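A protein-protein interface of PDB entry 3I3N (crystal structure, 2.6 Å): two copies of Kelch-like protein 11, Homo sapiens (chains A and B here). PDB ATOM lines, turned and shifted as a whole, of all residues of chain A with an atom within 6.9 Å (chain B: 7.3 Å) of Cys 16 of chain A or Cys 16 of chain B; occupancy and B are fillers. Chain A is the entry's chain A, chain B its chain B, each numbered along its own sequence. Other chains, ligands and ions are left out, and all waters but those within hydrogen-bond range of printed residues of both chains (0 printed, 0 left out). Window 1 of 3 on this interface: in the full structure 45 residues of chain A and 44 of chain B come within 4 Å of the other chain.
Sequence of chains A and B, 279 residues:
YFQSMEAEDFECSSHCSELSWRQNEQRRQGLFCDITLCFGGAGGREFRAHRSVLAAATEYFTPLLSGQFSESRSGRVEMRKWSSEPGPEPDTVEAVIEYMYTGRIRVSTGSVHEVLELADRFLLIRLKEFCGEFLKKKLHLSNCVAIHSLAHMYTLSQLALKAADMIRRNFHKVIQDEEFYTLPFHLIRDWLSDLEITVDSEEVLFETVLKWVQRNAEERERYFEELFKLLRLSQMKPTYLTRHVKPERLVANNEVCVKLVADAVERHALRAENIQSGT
His 15 of chain A touches Tyr 101 of chain B, and with the chains exchanged Tyr 101 of chain A touches His 15 of chain B. His 15 of chain A touches Thr 102 of chain B, and with the chains exchanged Thr 102 of chain A touches His 15 of chain B. Cys 16 of chain B touches its own counterpart, Cys 16 of chain A. Ser 17 of chain A touches Cys 16 of chain B, but with the chains exchanged Cys 16 of chain A does not touch Ser 17 of chain B (4.1 Å). Positions printed for both chains: 12, 13, 14, 15, 16, 17, 18, 19, 20, 21, 22, 23, 101, 102 and 103.
Of the printed residues of chain B, Ser 17 of chain A touches Cys 16. Arg 22 of chain A touches none of the printed residues of chain B. Printed residues of chain B within 4 Å of Gly 103 of chain A: Cys 12 and His 15. Of the printed residues of chain A, His 15 of chain B touches Tyr 101 (3.8 Å), Thr 102 (3.6 Å) and Gly 103 (3.3 Å). Cys 16 of chain B touches just these residues of chain A: Cys 16, Ser 17, Ser 20 and Thr 102. Glu 18 of chain B touches none of the printed residues of chain A. Of the printed residues of chain A, Leu 19 of chain B touches Tyr 101. Of the printed residues of chain A, Gly 103 of chain B touches Glu 11, Cys 12 and His 15. The nearest residue of chain B that does not touch Cys 16 of chain A is Ser 17 of chain B (4.1 Å). The nearest residue of chain A that does not touch Cys 16 of chain B is Tyr 101 of chain A (4.6 Å). The nearest printed residue of chain A that does not touch Thr 102 of chain B is Glu 11 of chain A (5.0 Å).
N of Arg 104 of chain B sits close to OG1 of Thr 102 of chain B (3.2 Å). The backbone carbonyl oxygen (O) of Ser 14 of chain A lies within hydrogen-bond range of the side-chain hydroxyl (OG) of Ser 17 of chain A, at 3.0 Å. OG of Ser 20 of chain A sits at hydrogen-bond distance from O of Tyr 101 of chain A, at 3.0 Å. The side-chain hydroxyl (OG) of Ser 20 of chain B is in hydrogen-bond range of the backbone carbonyl oxygen (O) of Ser 17 of chain B. The side-chain sulfur (SG) of Cys 12 of chain B is in hydrogen-bond range of the backbone NH (N) of His 15 of chain B (3.7 Å). OG of Ser 20 of chain B sits close to O of Tyr 101 of chain B (3.3 Å).
Among the printed residues, pairs that only touch across the chains: Glu 11 of chain A with Gly 103 of chain B (3.4 Å), Leu 19 of chain A with Tyr 101 of chain B (3.5 Å), Thr 102 of chain A with His 15 of chain B (3.6 Å), Tyr 101 of chain A with Leu 19 of chain B (3.6 Å), His 15 of chain A with Thr 102 of chain B (3.7 Å), Thr 102 of chain A with Cys 16 of chain B (3.8 Å), Cys 16 of chain A with Cys 16 of chain B (3.8 Å), Tyr 101 of chain A with His 15 of chain B (3.8 Å), Leu 19 of chain A with Ser 20 of chain B (3.9 Å), Cys 16 of chain A with Thr 102 of chain B (3.9 Å), Ser 17 of chain A with Cys 16 of chain B (3.97 Å) and His 15 of chain A with Tyr 101 of chain B (3.98 Å).
Hydrophobic or aromatic side chains of chain A that line the printed part of chain B: His 15 and Leu 19. Of the 16 printed residues of chain B, 10 touch a printed residue of chain A. Printed residues of chain B that touch a printed residue of chain A: Cys 12, His 15, Cys 16, Leu 19, Ser 20, Gln 23, Tyr 101, Thr 102, Gly 103 and Arg 104. Hydrophobic or aromatic side chains of chain B within 4 Å of the printed part of chain A: His 15 and Leu 19. Along chain B the printed residues that touch a printed residue of chain A span positions 12 to 104. Among the printed residues, Asp or Glu carboxylates within 4 Å of a Lys or Arg side-chain nitrogen of the other chain: Glu 11 of chain A with Arg 104 of chain B.
SG of Cys 16 of chain B is in hydrogen-bond range of OG of Ser 20 of chain A. The side-chain amide oxygen (OE1) of Gln 23 of chain A sits at hydrogen-bond distance from the side-chain amide nitrogen (NE2) of Gln 23 of chain B, at 2.9 Å. N of Gly 103 of chain B sits at hydrogen-bond distance from ND1 of His 15 of chain A, 3.5 Å away. The backbone NH (N) of Cys 12 of chain A lies within hydrogen-bond range of the backbone carbonyl oxygen (O) of Gly 103 of chain B (3.0 Å). The backbone carbonyl oxygen (O) of Gly 103 of chain A lies within hydrogen-bond range of the backbone NH (N) of Cys 12 of chain B. The side-chain hydroxyl (OG) of Ser 20 of chain B is in hydrogen-bond range of the side-chain sulfur (SG) of Cys 16 of chain A (3.1 Å). OE2 of Glu 11 of chain A lies within salt-bridge range of NE of Arg 104 of chain B, at 3.5 Å. ND1 of His 15 of chain B sits at hydrogen-bond distance from N of Gly 103 of chain A, at 3.3 Å.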
ATOM      1  N   GLU A  11     -21.088  17.055 -36.892  1.00  0.00           N
ATOM      2  CA  GLU A  11     -21.711  16.146 -35.959  1.00  0.00           C
ATOM      3  C   GLU A  11     -21.118  16.381 -34.596  1.00  0.00           C
ATOM      4  O   GLU A  11     -19.931  16.166 -34.371  1.00  0.00           O
ATOM      5  CB  GLU A  11     -21.507  14.685 -36.387  1.00  0.00           C
ATOM      6  CG  GLU A  11     -21.873  13.673 -35.303  1.00  0.00           C
ATOM      7  CD  GLU A  11     -22.552  12.412 -35.840  1.00  0.00           C
ATOM      8  OE1 GLU A  11     -21.944  11.714 -36.687  1.00  0.00           O
ATOM      9  OE2 GLU A  11     -23.696  12.122 -35.403  1.00  0.00           O
ATOM     10  N   CYS A  12     -21.959  16.865 -33.696  1.00  0.00           N
ATOM     11  CA  CYS A  12     -21.557  17.117 -32.327  1.00  0.00           C
ATOM     12  C   CYS A  12     -21.793  15.789 -31.599  1.00  0.00           C
ATOM     13  O   CYS A  12     -22.900  15.490 -31.150  1.00  0.00           O
ATOM     14  CB  CYS A  12     -22.418  18.228 -31.754  1.00  0.00           C
ATOM     15  SG  CYS A  12     -22.094  18.527 -30.056  1.00  0.00           S
ATOM     16  N   SER A  13     -20.728  15.000 -31.508  1.00  0.00           N
ATOM     17  CA  SER A  13     -20.742  13.662 -30.914  1.00  0.00           C
ATOM     18  C   SER A  13     -21.334  13.442 -29.524  1.00  0.00           C
ATOM     19  O   SER A  13     -21.662  12.302 -29.183  1.00  0.00           O
ATOM     20  CB  SER A  13     -19.329  13.088 -30.920  1.00  0.00           C
ATOM     21  OG  SER A  13     -18.518  13.778 -29.979  1.00  0.00           O
ATOM     22  N   SER A  14     -21.476  14.490 -28.718  1.00  0.00           N
ATOM     23  CA  SER A  14     -22.027  14.305 -27.376  1.00  0.00           C
ATOM     24  C   SER A  14     -23.448  14.876 -27.220  1.00  0.00           C
ATOM     25  O   SER A  14     -24.060  14.792 -26.141  1.00  0.00           O
ATOM     26  CB  SER A  14     -21.099  14.957 -26.349  1.00  0.00           C
ATOM     27  OG  SER A  14     -21.136  16.368 -26.477  1.00  0.00           O
ATOM     28  N   HIS A  15     -23.967  15.429 -28.316  1.00  0.00           N
ATOM     29  CA  HIS A  15     -25.279  16.061 -28.356  1.00  0.00           C
ATOM     30  C   HIS A  15     -26.470  15.292 -27.785  1.00  0.00           C
ATOM     31  O   HIS A  15     -27.206  15.807 -26.946  1.00  0.00           O
ATOM     32  CB  HIS A  15     -25.585  16.483 -29.800  1.00  0.00           C
ATOM     33  CG  HIS A  15     -26.837  17.284 -29.932  1.00  0.00           C
ATOM     34  ND1 HIS A  15     -28.092  16.710 -29.925  1.00  0.00           N
ATOM     35  CD2 HIS A  15     -27.032  18.622 -30.006  1.00  0.00           C
ATOM     36  CE1 HIS A  15     -29.007  17.661 -29.987  1.00  0.00           C
ATOM     37  NE2 HIS A  15     -28.391  18.831 -30.038  1.00  0.00           N
ATOM     38  N   CYS A  16     -26.669  14.066 -28.246  1.00  0.00           N
ATOM     39  CA  CYS A  16     -27.787  13.252 -27.797  1.00  0.00           C
ATOM     40  C   CYS A  16     -27.759  12.863 -26.316  1.00  0.00           C
ATOM     41  O   CYS A  16     -28.762  13.001 -25.608  1.00  0.00           O
ATOM     42  CB  CYS A  16     -27.888  12.014 -28.686  1.00  0.00           C
ATOM     43  SG  CYS A  16     -28.098  12.460 -30.451  1.00  0.00           S
ATOM     44  N   SER A  17     -26.625  12.382 -25.827  1.00  0.00           N
ATOM     45  CA  SER A  17     -26.561  12.024 -24.414  1.00  0.00           C
ATOM     46  C   SER A  17     -26.853  13.270 -23.543  1.00  0.00           C
ATOM     47  O   SER A  17     -27.541  13.170 -22.525  1.00  0.00           O
ATOM     48  CB  SER A  17     -25.196  11.431 -24.087  1.00  0.00           C
ATOM     49  OG  SER A  17     -24.185  12.371 -24.388  1.00  0.00           O
ATOM     50  N   GLU A  18     -26.355  14.439 -23.951  1.00  0.00           N
ATOM     51  CA  GLU A  18     -26.620  15.684 -23.210  1.00  0.00           C
ATOM     52  C   GLU A  18     -28.104  16.063 -23.324  1.00  0.00           C
ATOM     53  O   GLU A  18     -28.712  16.595 -22.393  1.00  0.00           O
ATOM     54  CB  GLU A  18     -25.794  16.842 -23.771  1.00  0.00           C
ATOM     55  CG  GLU A  18     -24.321  16.817 -23.444  1.00  0.00           C
ATOM     56  CD  GLU A  18     -23.558  17.925 -24.157  1.00  0.00           C
ATOM     57  OE1 GLU A  18     -23.416  17.863 -25.404  1.00  0.00           O
ATOM     58  OE2 GLU A  18     -23.105  18.870 -23.473  1.00  0.00           O
ATOM     59  N   LEU A  19     -28.677  15.793 -24.487  1.00  0.00           N
ATOM     60  CA  LEU A  19     -30.068  16.109 -24.731  1.00  0.00           C
ATOM     61  C   LEU A  19     -30.959  15.251 -23.853  1.00  0.00           C
ATOM     62  O   LEU A  19     -31.815  15.750 -23.121  1.00  0.00           O
ATOM     63  CB  LEU A  19     -30.393  15.854 -26.208  1.00  0.00           C
ATOM     64  CG  LEU A  19     -31.729  16.368 -26.737  1.00  0.00           C
ATOM     65  CD1 LEU A  19     -31.734  17.899 -26.749  1.00  0.00           C
ATOM     66  CD2 LEU A  19     -31.936  15.827 -28.141  1.00  0.00           C
ATOM     67  N   SER A  20     -30.760  13.946 -23.940  1.00  0.00           N
ATOM     68  CA  SER A  20     -31.578  13.037 -23.160  1.00  0.00           C
ATOM     69  C   SER A  20     -31.351  13.296 -21.666  1.00  0.00           C
ATOM     70  O   SER A  20     -32.241  13.099 -20.855  1.00  0.00           O
ATOM     71  CB  SER A  20     -31.255  11.581 -23.537  1.00  0.00           C
ATOM     72  OG  SER A  20     -30.430  10.969 -22.568  1.00  0.00           O
ATOM     73  N   TRP A  21     -30.165  13.773 -21.313  1.00  0.00           N
ATOM     74  CA  TRP A  21     -29.874  14.071 -19.925  1.00  0.00           C
ATOM     75  C   TRP A  21     -30.710  15.255 -19.435  1.00  0.00           C
ATOM     76  O   TRP A  21     -31.360  15.179 -18.384  1.00  0.00           O
ATOM     77  CB  TRP A  21     -28.385  14.376 -19.744  1.00  0.00           C
ATOM     78  CG  TRP A  21     -28.032  14.565 -18.301  1.00  0.00           C
ATOM     79  CD1 TRP A  21     -27.734  15.750 -17.665  1.00  0.00           C
ATOM     80  CD2 TRP A  21     -28.066  13.557 -17.280  1.00  0.00           C
ATOM     81  NE1 TRP A  21     -27.584  15.535 -16.314  1.00  0.00           N
ATOM     82  CE2 TRP A  21     -27.771  14.201 -16.049  1.00  0.00           C
ATOM     83  CE3 TRP A  21     -28.296  12.166 -17.287  1.00  0.00           C
ATOM     84  CZ2 TRP A  21     -27.731  13.499 -14.827  1.00  0.00           C
ATOM     85  CZ3 TRP A  21     -28.254  11.468 -16.072  1.00  0.00           C
ATOM     86  CH2 TRP A  21     -27.964  12.138 -14.863  1.00  0.00           C
ATOM     87  N   ARG A  22     -30.699  16.348 -20.190  1.00  0.00           N
ATOM     88  CA  ARG A  22     -31.478  17.532 -19.818  1.00  0.00           C
ATOM     89  C   ARG A  22     -32.997  17.299 -19.823  1.00  0.00           C
ATOM     90  O   ARG A  22     -33.730  17.959 -19.084  1.00  0.00           O
ATOM     91  CB  ARG A  22     -31.122  18.695 -20.730  1.00  0.00           C
ATOM     92  CG  ARG A  22     -29.649  18.999 -20.722  1.00  0.00           C
ATOM     93  CD  ARG A  22     -29.337  20.308 -21.419  1.00  0.00           C
ATOM     94  NE  ARG A  22     -30.252  21.368 -21.001  1.00  0.00           N
ATOM     95  CZ  ARG A  22     -29.996  22.669 -21.121  1.00  0.00           C
ATOM     96  NH1 ARG A  22     -28.841  23.078 -21.637  1.00  0.00           N
ATOM     97  NH2 ARG A  22     -30.903  23.566 -20.744  1.00  0.00           N
ATOM     98  N   GLN A  23     -33.479  16.372 -20.649  1.00  0.00           N
ATOM     99  CA  GLN A  23     -34.914  16.100 -20.671  1.00  0.00           C
ATOM    100  C   GLN A  23     -35.226  15.321 -19.409  1.00  0.00           C
ATOM    101  O   GLN A  23     -36.365  15.294 -18.944  1.00  0.00           O
ATOM    102  CB  GLN A  23     -35.333  15.288 -21.910  1.00  0.00           C
ATOM    103  CG  GLN A  23     -35.353  16.080 -23.215  1.00  0.00           C
ATOM    104  CD  GLN A  23     -35.783  15.235 -24.422  1.00  0.00           C
ATOM    105  OE1 GLN A  23     -36.939  15.253 -24.825  1.00  0.00           O
ATOM    106  NE2 GLN A  23     -34.846  14.485 -24.986  1.00  0.00           N
ATOM    107  N   TYR A 101     -35.564   7.419 -20.414  1.00  0.00           N
ATOM    108  CA  TYR A 101     -34.899   8.661 -20.796  1.00  0.00           C
ATOM    109  C   TYR A 101     -33.394   8.575 -20.989  1.00  0.00           C
ATOM    110  O   TYR A 101     -32.832   9.334 -21.751  1.00  0.00           O
ATOM    111  CB  TYR A 101     -35.100   9.731 -19.745  1.00  0.00           C
ATOM    112  CG  TYR A 101     -36.429  10.423 -19.742  1.00  0.00           C
ATOM    113  CD1 TYR A 101     -37.600   9.715 -19.557  1.00  0.00           C
ATOM    114  CD2 TYR A 101     -36.506  11.807 -19.900  1.00  0.00           C
ATOM    115  CE1 TYR A 101     -38.836  10.378 -19.525  1.00  0.00           C
ATOM    116  CE2 TYR A 101     -37.735  12.480 -19.877  1.00  0.00           C
ATOM    117  CZ  TYR A 101     -38.888  11.759 -19.687  1.00  0.00           C
ATOM    118  OH  TYR A 101     -40.099  12.414 -19.647  1.00  0.00           O
ATOM    119  N   THR A 102     -32.714   7.657 -20.311  1.00  0.00           N
ATOM    120  CA  THR A 102     -31.250   7.656 -20.415  1.00  0.00           C
ATOM    121  C   THR A 102     -30.581   6.364 -20.802  1.00  0.00           C
ATOM    122  O   THR A 102     -29.368   6.351 -21.005  1.00  0.00           O
ATOM    123  CB  THR A 102     -30.615   8.028 -19.072  1.00  0.00           C
ATOM    124  OG1 THR A 102     -30.888   6.964 -18.151  1.00  0.00           O
ATOM    125  CG2 THR A 102     -31.197   9.309 -18.504  1.00  0.00           C
ATOM    126  N   GLY A 103     -31.327   5.282 -20.886  1.00  0.00           N
ATOM    127  CA  GLY A 103     -30.668   4.029 -21.198  1.00  0.00           C
ATOM    128  C   GLY A 103     -29.745   3.498 -20.075  1.00  0.00           C
ATOM    129  O   GLY A 103     -28.971   2.582 -20.337  1.00  0.00           O
ATOM    130  N   CYS B  12     -27.165   0.968 -21.935  1.00  0.00           N
ATOM    131  CA  CYS B  12     -27.387   0.742 -23.360  1.00  0.00           C
ATOM    132  C   CYS B  12     -26.667   1.860 -24.131  1.00  0.00           C
ATOM    133  O   CYS B  12     -27.131   3.005 -24.178  1.00  0.00           O
ATOM    134  CB  CYS B  12     -28.880   0.753 -23.665  1.00  0.00           C
ATOM    135  SG  CYS B  12     -29.261   0.289 -25.362  1.00  0.00           S
ATOM    136  N   SER B  13     -25.529   1.525 -24.727  1.00  0.00           N
ATOM    137  CA  SER B  13     -24.727   2.514 -25.443  1.00  0.00           C
ATOM    138  C   SER B  13     -25.403   3.274 -26.593  1.00  0.00           C
ATOM    139  O   SER B  13     -25.085   4.444 -26.817  1.00  0.00           O
ATOM    140  CB  SER B  13     -23.436   1.862 -25.964  1.00  0.00           C
ATOM    141  OG  SER B  13     -23.726   0.798 -26.859  1.00  0.00           O
ATOM    142  N   SER B  14     -26.322   2.642 -27.326  1.00  0.00           N
ATOM    143  CA  SER B  14     -26.954   3.358 -28.428  1.00  0.00           C
ATOM    144  C   SER B  14     -28.245   4.085 -28.005  1.00  0.00           C
ATOM    145  O   SER B  14     -28.656   5.064 -28.620  1.00  0.00           O
ATOM    146  CB  SER B  14     -27.236   2.395 -29.592  1.00  0.00           C
ATOM    147  OG  SER B  14     -28.264   1.480 -29.263  1.00  0.00           O
ATOM    148  N   HIS B  15     -28.862   3.637 -26.925  1.00  0.00           N
ATOM    149  CA  HIS B  15     -30.105   4.245 -26.474  1.00  0.00           C
ATOM    150  C   HIS B  15     -30.337   5.769 -26.681  1.00  0.00           C
ATOM    151  O   HIS B  15     -31.389   6.162 -27.159  1.00  0.00           O
ATOM    152  CB  HIS B  15     -30.336   3.872 -24.997  1.00  0.00           C
ATOM    153  CG  HIS B  15     -31.638   4.365 -24.437  1.00  0.00           C
ATOM    154  ND1 HIS B  15     -31.836   5.682 -24.074  1.00  0.00           N
ATOM    155  CD2 HIS B  15     -32.814   3.728 -24.206  1.00  0.00           C
ATOM    156  CE1 HIS B  15     -33.082   5.838 -23.642  1.00  0.00           C
ATOM    157  NE2 HIS B  15     -33.699   4.669 -23.713  1.00  0.00           N
ATOM    158  N   CYS B  16     -29.381   6.624 -26.336  1.00  0.00           N
ATOM    159  CA  CYS B  16     -29.640   8.056 -26.468  1.00  0.00           C
ATOM    160  C   CYS B  16     -29.771   8.549 -27.892  1.00  0.00           C
ATOM    161  O   CYS B  16     -30.613   9.399 -28.192  1.00  0.00           O
ATOM    162  CB  CYS B  16     -28.581   8.861 -25.712  1.00  0.00           C
ATOM    163  SG  CYS B  16     -28.802   8.757 -23.899  1.00  0.00           S
ATOM    164  N   SER B  17     -28.946   8.017 -28.777  1.00  0.00           N
ATOM    165  CA  SER B  17     -29.022   8.392 -30.172  1.00  0.00           C
ATOM    166  C   SER B  17     -30.380   7.978 -30.676  1.00  0.00           C
ATOM    167  O   SER B  17     -31.088   8.769 -31.278  1.00  0.00           O
ATOM    168  CB  SER B  17     -27.941   7.678 -30.982  1.00  0.00           C
ATOM    169  OG  SER B  17     -26.702   8.344 -30.825  1.00  0.00           O
ATOM    170  N   GLU B  18     -30.748   6.732 -30.402  1.00  0.00           N
ATOM    171  CA  GLU B  18     -32.023   6.204 -30.854  1.00  0.00           C
ATOM    172  C   GLU B  18     -33.186   7.012 -30.329  1.00  0.00           C
ATOM    173  O   GLU B  18     -34.167   7.227 -31.032  1.00  0.00           O
ATOM    174  CB  GLU B  18     -32.182   4.750 -30.426  1.00  0.00           C
ATOM    175  CG  GLU B  18     -30.940   3.917 -30.657  1.00  0.00           C
ATOM    176  CD  GLU B  18     -31.243   2.419 -30.795  1.00  0.00           C
ATOM    177  OE1 GLU B  18     -32.213   1.930 -30.155  1.00  0.00           O
ATOM    178  OE2 GLU B  18     -30.499   1.730 -31.542  1.00  0.00           O
ATOM    179  N   LEU B  19     -33.077   7.473 -29.092  1.00  0.00           N
ATOM    180  CA  LEU B  19     -34.148   8.252 -28.499  1.00  0.00           C
ATOM    181  C   LEU B  19     -34.332   9.560 -29.248  1.00  0.00           C
ATOM    182  O   LEU B  19     -35.427   9.901 -29.660  1.00  0.00           O
ATOM    183  CB  LEU B  19     -33.844   8.579 -27.035  1.00  0.00           C
ATOM    184  CG  LEU B  19     -35.073   8.876 -26.160  1.00  0.00           C
ATOM    185  CD1 LEU B  19     -35.837   7.559 -25.893  1.00  0.00           C
ATOM    186  CD2 LEU B  19     -34.636   9.508 -24.836  1.00  0.00           C
ATOM    187  N   SER B  20     -33.245  10.287 -29.437  1.00  0.00           N
ATOM    188  CA  SER B  20     -33.362  11.562 -30.088  1.00  0.00           C
ATOM    189  C   SER B  20     -33.724  11.433 -31.579  1.00  0.00           C
ATOM    190  O   SER B  20     -34.339  12.335 -32.143  1.00  0.00           O
ATOM    191  CB  SER B  20     -32.078  12.364 -29.890  1.00  0.00           C
ATOM    192  OG  SER B  20     -31.110  11.970 -30.835  1.00  0.00           O
ATOM    193  N   TRP B  21     -33.374  10.317 -32.211  1.00  0.00           N
ATOM    194  CA  TRP B  21     -33.726  10.171 -33.611  1.00  0.00           C
ATOM    195  C   TRP B  21     -35.207   9.872 -33.769  1.00  0.00           C
ATOM    196  O   TRP B  21     -35.846  10.359 -34.708  1.00  0.00           O
ATOM    197  CB  TRP B  21     -32.857   9.116 -34.300  1.00  0.00           C
ATOM    198  CG  TRP B  21     -31.510   9.700 -34.672  1.00  0.00           C
ATOM    199  CD1 TRP B  21     -30.402   9.811 -33.864  1.00  0.00           C
ATOM    200  CD2 TRP B  21     -31.177  10.398 -35.889  1.00  0.00           C
ATOM    201  NE1 TRP B  21     -29.412  10.539 -34.496  1.00  0.00           N
ATOM    202  CE2 TRP B  21     -29.858  10.908 -35.737  1.00  0.00           C
ATOM    203  CE3 TRP B  21     -31.865  10.645 -37.090  1.00  0.00           C
ATOM    204  CZ2 TRP B  21     -29.220  11.653 -36.740  1.00  0.00           C
ATOM    205  CZ3 TRP B  21     -31.228  11.388 -38.089  1.00  0.00           C
ATOM    206  CH2 TRP B  21     -29.917  11.881 -37.905  1.00  0.00           C
ATOM    207  N   ARG B  22     -35.768   9.091 -32.849  1.00  0.00           N
ATOM    208  CA  ARG B  22     -37.184   8.775 -32.932  1.00  0.00           C
ATOM    209  C   ARG B  22     -37.977  10.015 -32.628  1.00  0.00           C
ATOM    210  O   ARG B  22     -38.979  10.285 -33.288  1.00  0.00           O
ATOM    211  CB  ARG B  22     -37.546   7.631 -31.986  1.00  0.00           C
ATOM    212  CG  ARG B  22     -36.844   6.378 -32.409  1.00  0.00           C
ATOM    213  CD  ARG B  22     -37.175   5.156 -31.586  1.00  0.00           C
ATOM    214  NE  ARG B  22     -36.178   4.118 -31.860  1.00  0.00           N
ATOM    215  CZ  ARG B  22     -36.160   2.906 -31.310  1.00  0.00           C
ATOM    216  NH1 ARG B  22     -37.098   2.539 -30.435  1.00  0.00           N
ATOM    217  NH2 ARG B  22     -35.184   2.064 -31.627  1.00  0.00           N
ATOM    218  N   GLN B  23     -37.542  10.801 -31.649  1.00  0.00           N
ATOM    219  CA  GLN B  23     -38.288  12.035 -31.398  1.00  0.00           C
ATOM    220  C   GLN B  23     -38.269  12.898 -32.699  1.00  0.00           C
ATOM    221  O   GLN B  23     -39.219  13.615 -32.973  1.00  0.00           O
ATOM    222  CB  GLN B  23     -37.711  12.840 -30.210  1.00  0.00           C
ATOM    223  CG  GLN B  23     -37.990  12.178 -28.825  1.00  0.00           C
ATOM    224  CD  GLN B  23     -37.402  12.992 -27.662  1.00  0.00           C
ATOM    225  OE1 GLN B  23     -36.184  13.034 -27.491  1.00  0.00           O
ATOM    226  NE2 GLN B  23     -38.255  13.676 -26.903  1.00  0.00           N
ATOM    227  N   TYR B 101     -32.495  18.432 -32.706  1.00  0.00           N
ATOM    228  CA  TYR B 101     -32.915  17.096 -32.291  1.00  0.00           C
ATOM    229  C   TYR B 101     -31.789  16.088 -32.362  1.00  0.00           C
ATOM    230  O   TYR B 101     -31.733  15.172 -31.554  1.00  0.00           O
ATOM    231  CB  TYR B 101     -34.077  16.554 -33.165  1.00  0.00           C
ATOM    232  CG  TYR B 101     -35.467  17.068 -32.797  1.00  0.00           C
ATOM    233  CD1 TYR B 101     -35.724  18.443 -32.688  1.00  0.00           C
ATOM    234  CD2 TYR B 101     -36.491  16.181 -32.480  1.00  0.00           C
ATOM    235  CE1 TYR B 101     -36.968  18.915 -32.242  1.00  0.00           C
ATOM    236  CE2 TYR B 101     -37.749  16.642 -32.046  1.00  0.00           C
ATOM    237  CZ  TYR B 101     -37.962  18.002 -31.921  1.00  0.00           C
ATOM    238  OH  TYR B 101     -39.155  18.449 -31.401  1.00  0.00           O
ATOM    239  N   THR B 102     -30.869  16.263 -33.303  1.00  0.00           N
ATOM    240  CA  THR B 102     -29.830  15.254 -33.496  1.00  0.00           C
ATOM    241  C   THR B 102     -28.377  15.649 -33.451  1.00  0.00           C
ATOM    242  O   THR B 102     -27.508  14.784 -33.535  1.00  0.00           O
ATOM    243  CB  THR B 102     -29.990  14.566 -34.865  1.00  0.00           C
ATOM    244  OG1 THR B 102     -29.555  15.468 -35.892  1.00  0.00           O
ATOM    245  CG2 THR B 102     -31.442  14.173 -35.108  1.00  0.00           C
ATOM    246  N   GLY B 103     -28.093  16.935 -33.369  1.00  0.00           N
ATOM    247  CA  GLY B 103     -26.707  17.352 -33.349  1.00  0.00           C
ATOM    248  C   GLY B 103     -25.980  17.103 -34.666  1.00  0.00           C
ATOM    249  O   GLY B 103     -24.756  17.155 -34.690  1.00  0.00           O
ATOM    250  N   ARG B 104     -26.699  16.829 -35.759  1.00  0.00           N
ATOM    251  CA  ARG B 104     -26.047  16.587 -37.060  1.00  0.00           C
ATOM    252  C   ARG B 104     -26.613  17.544 -38.090  1.00  0.00           C
ATOM    253  O   ARG B 104     -27.821  17.765 -38.135  1.00  0.00           O
ATOM    254  CB  ARG B 104     -26.285  15.160 -37.590  1.00  0.00           C
ATOM    255  CG  ARG B 104     -25.682  14.009 -36.803  1.00  0.00           C
ATOM    256  CD  ARG B 104     -26.101  12.656 -37.410  1.00  0.00           C
ATOM    257  NE  ARG B 104     -25.237  12.227 -38.516  1.00  0.00           N
ATOM    258  CZ  ARG B 104     -25.675  11.790 -39.703  1.00  0.00           C
ATOM    259  NH1 ARG B 104     -26.981  11.721 -39.958  1.00  0.00           N
ATOM    260  NH2 ARG B 104     -24.803  11.420 -40.641  1.00  0.00           N
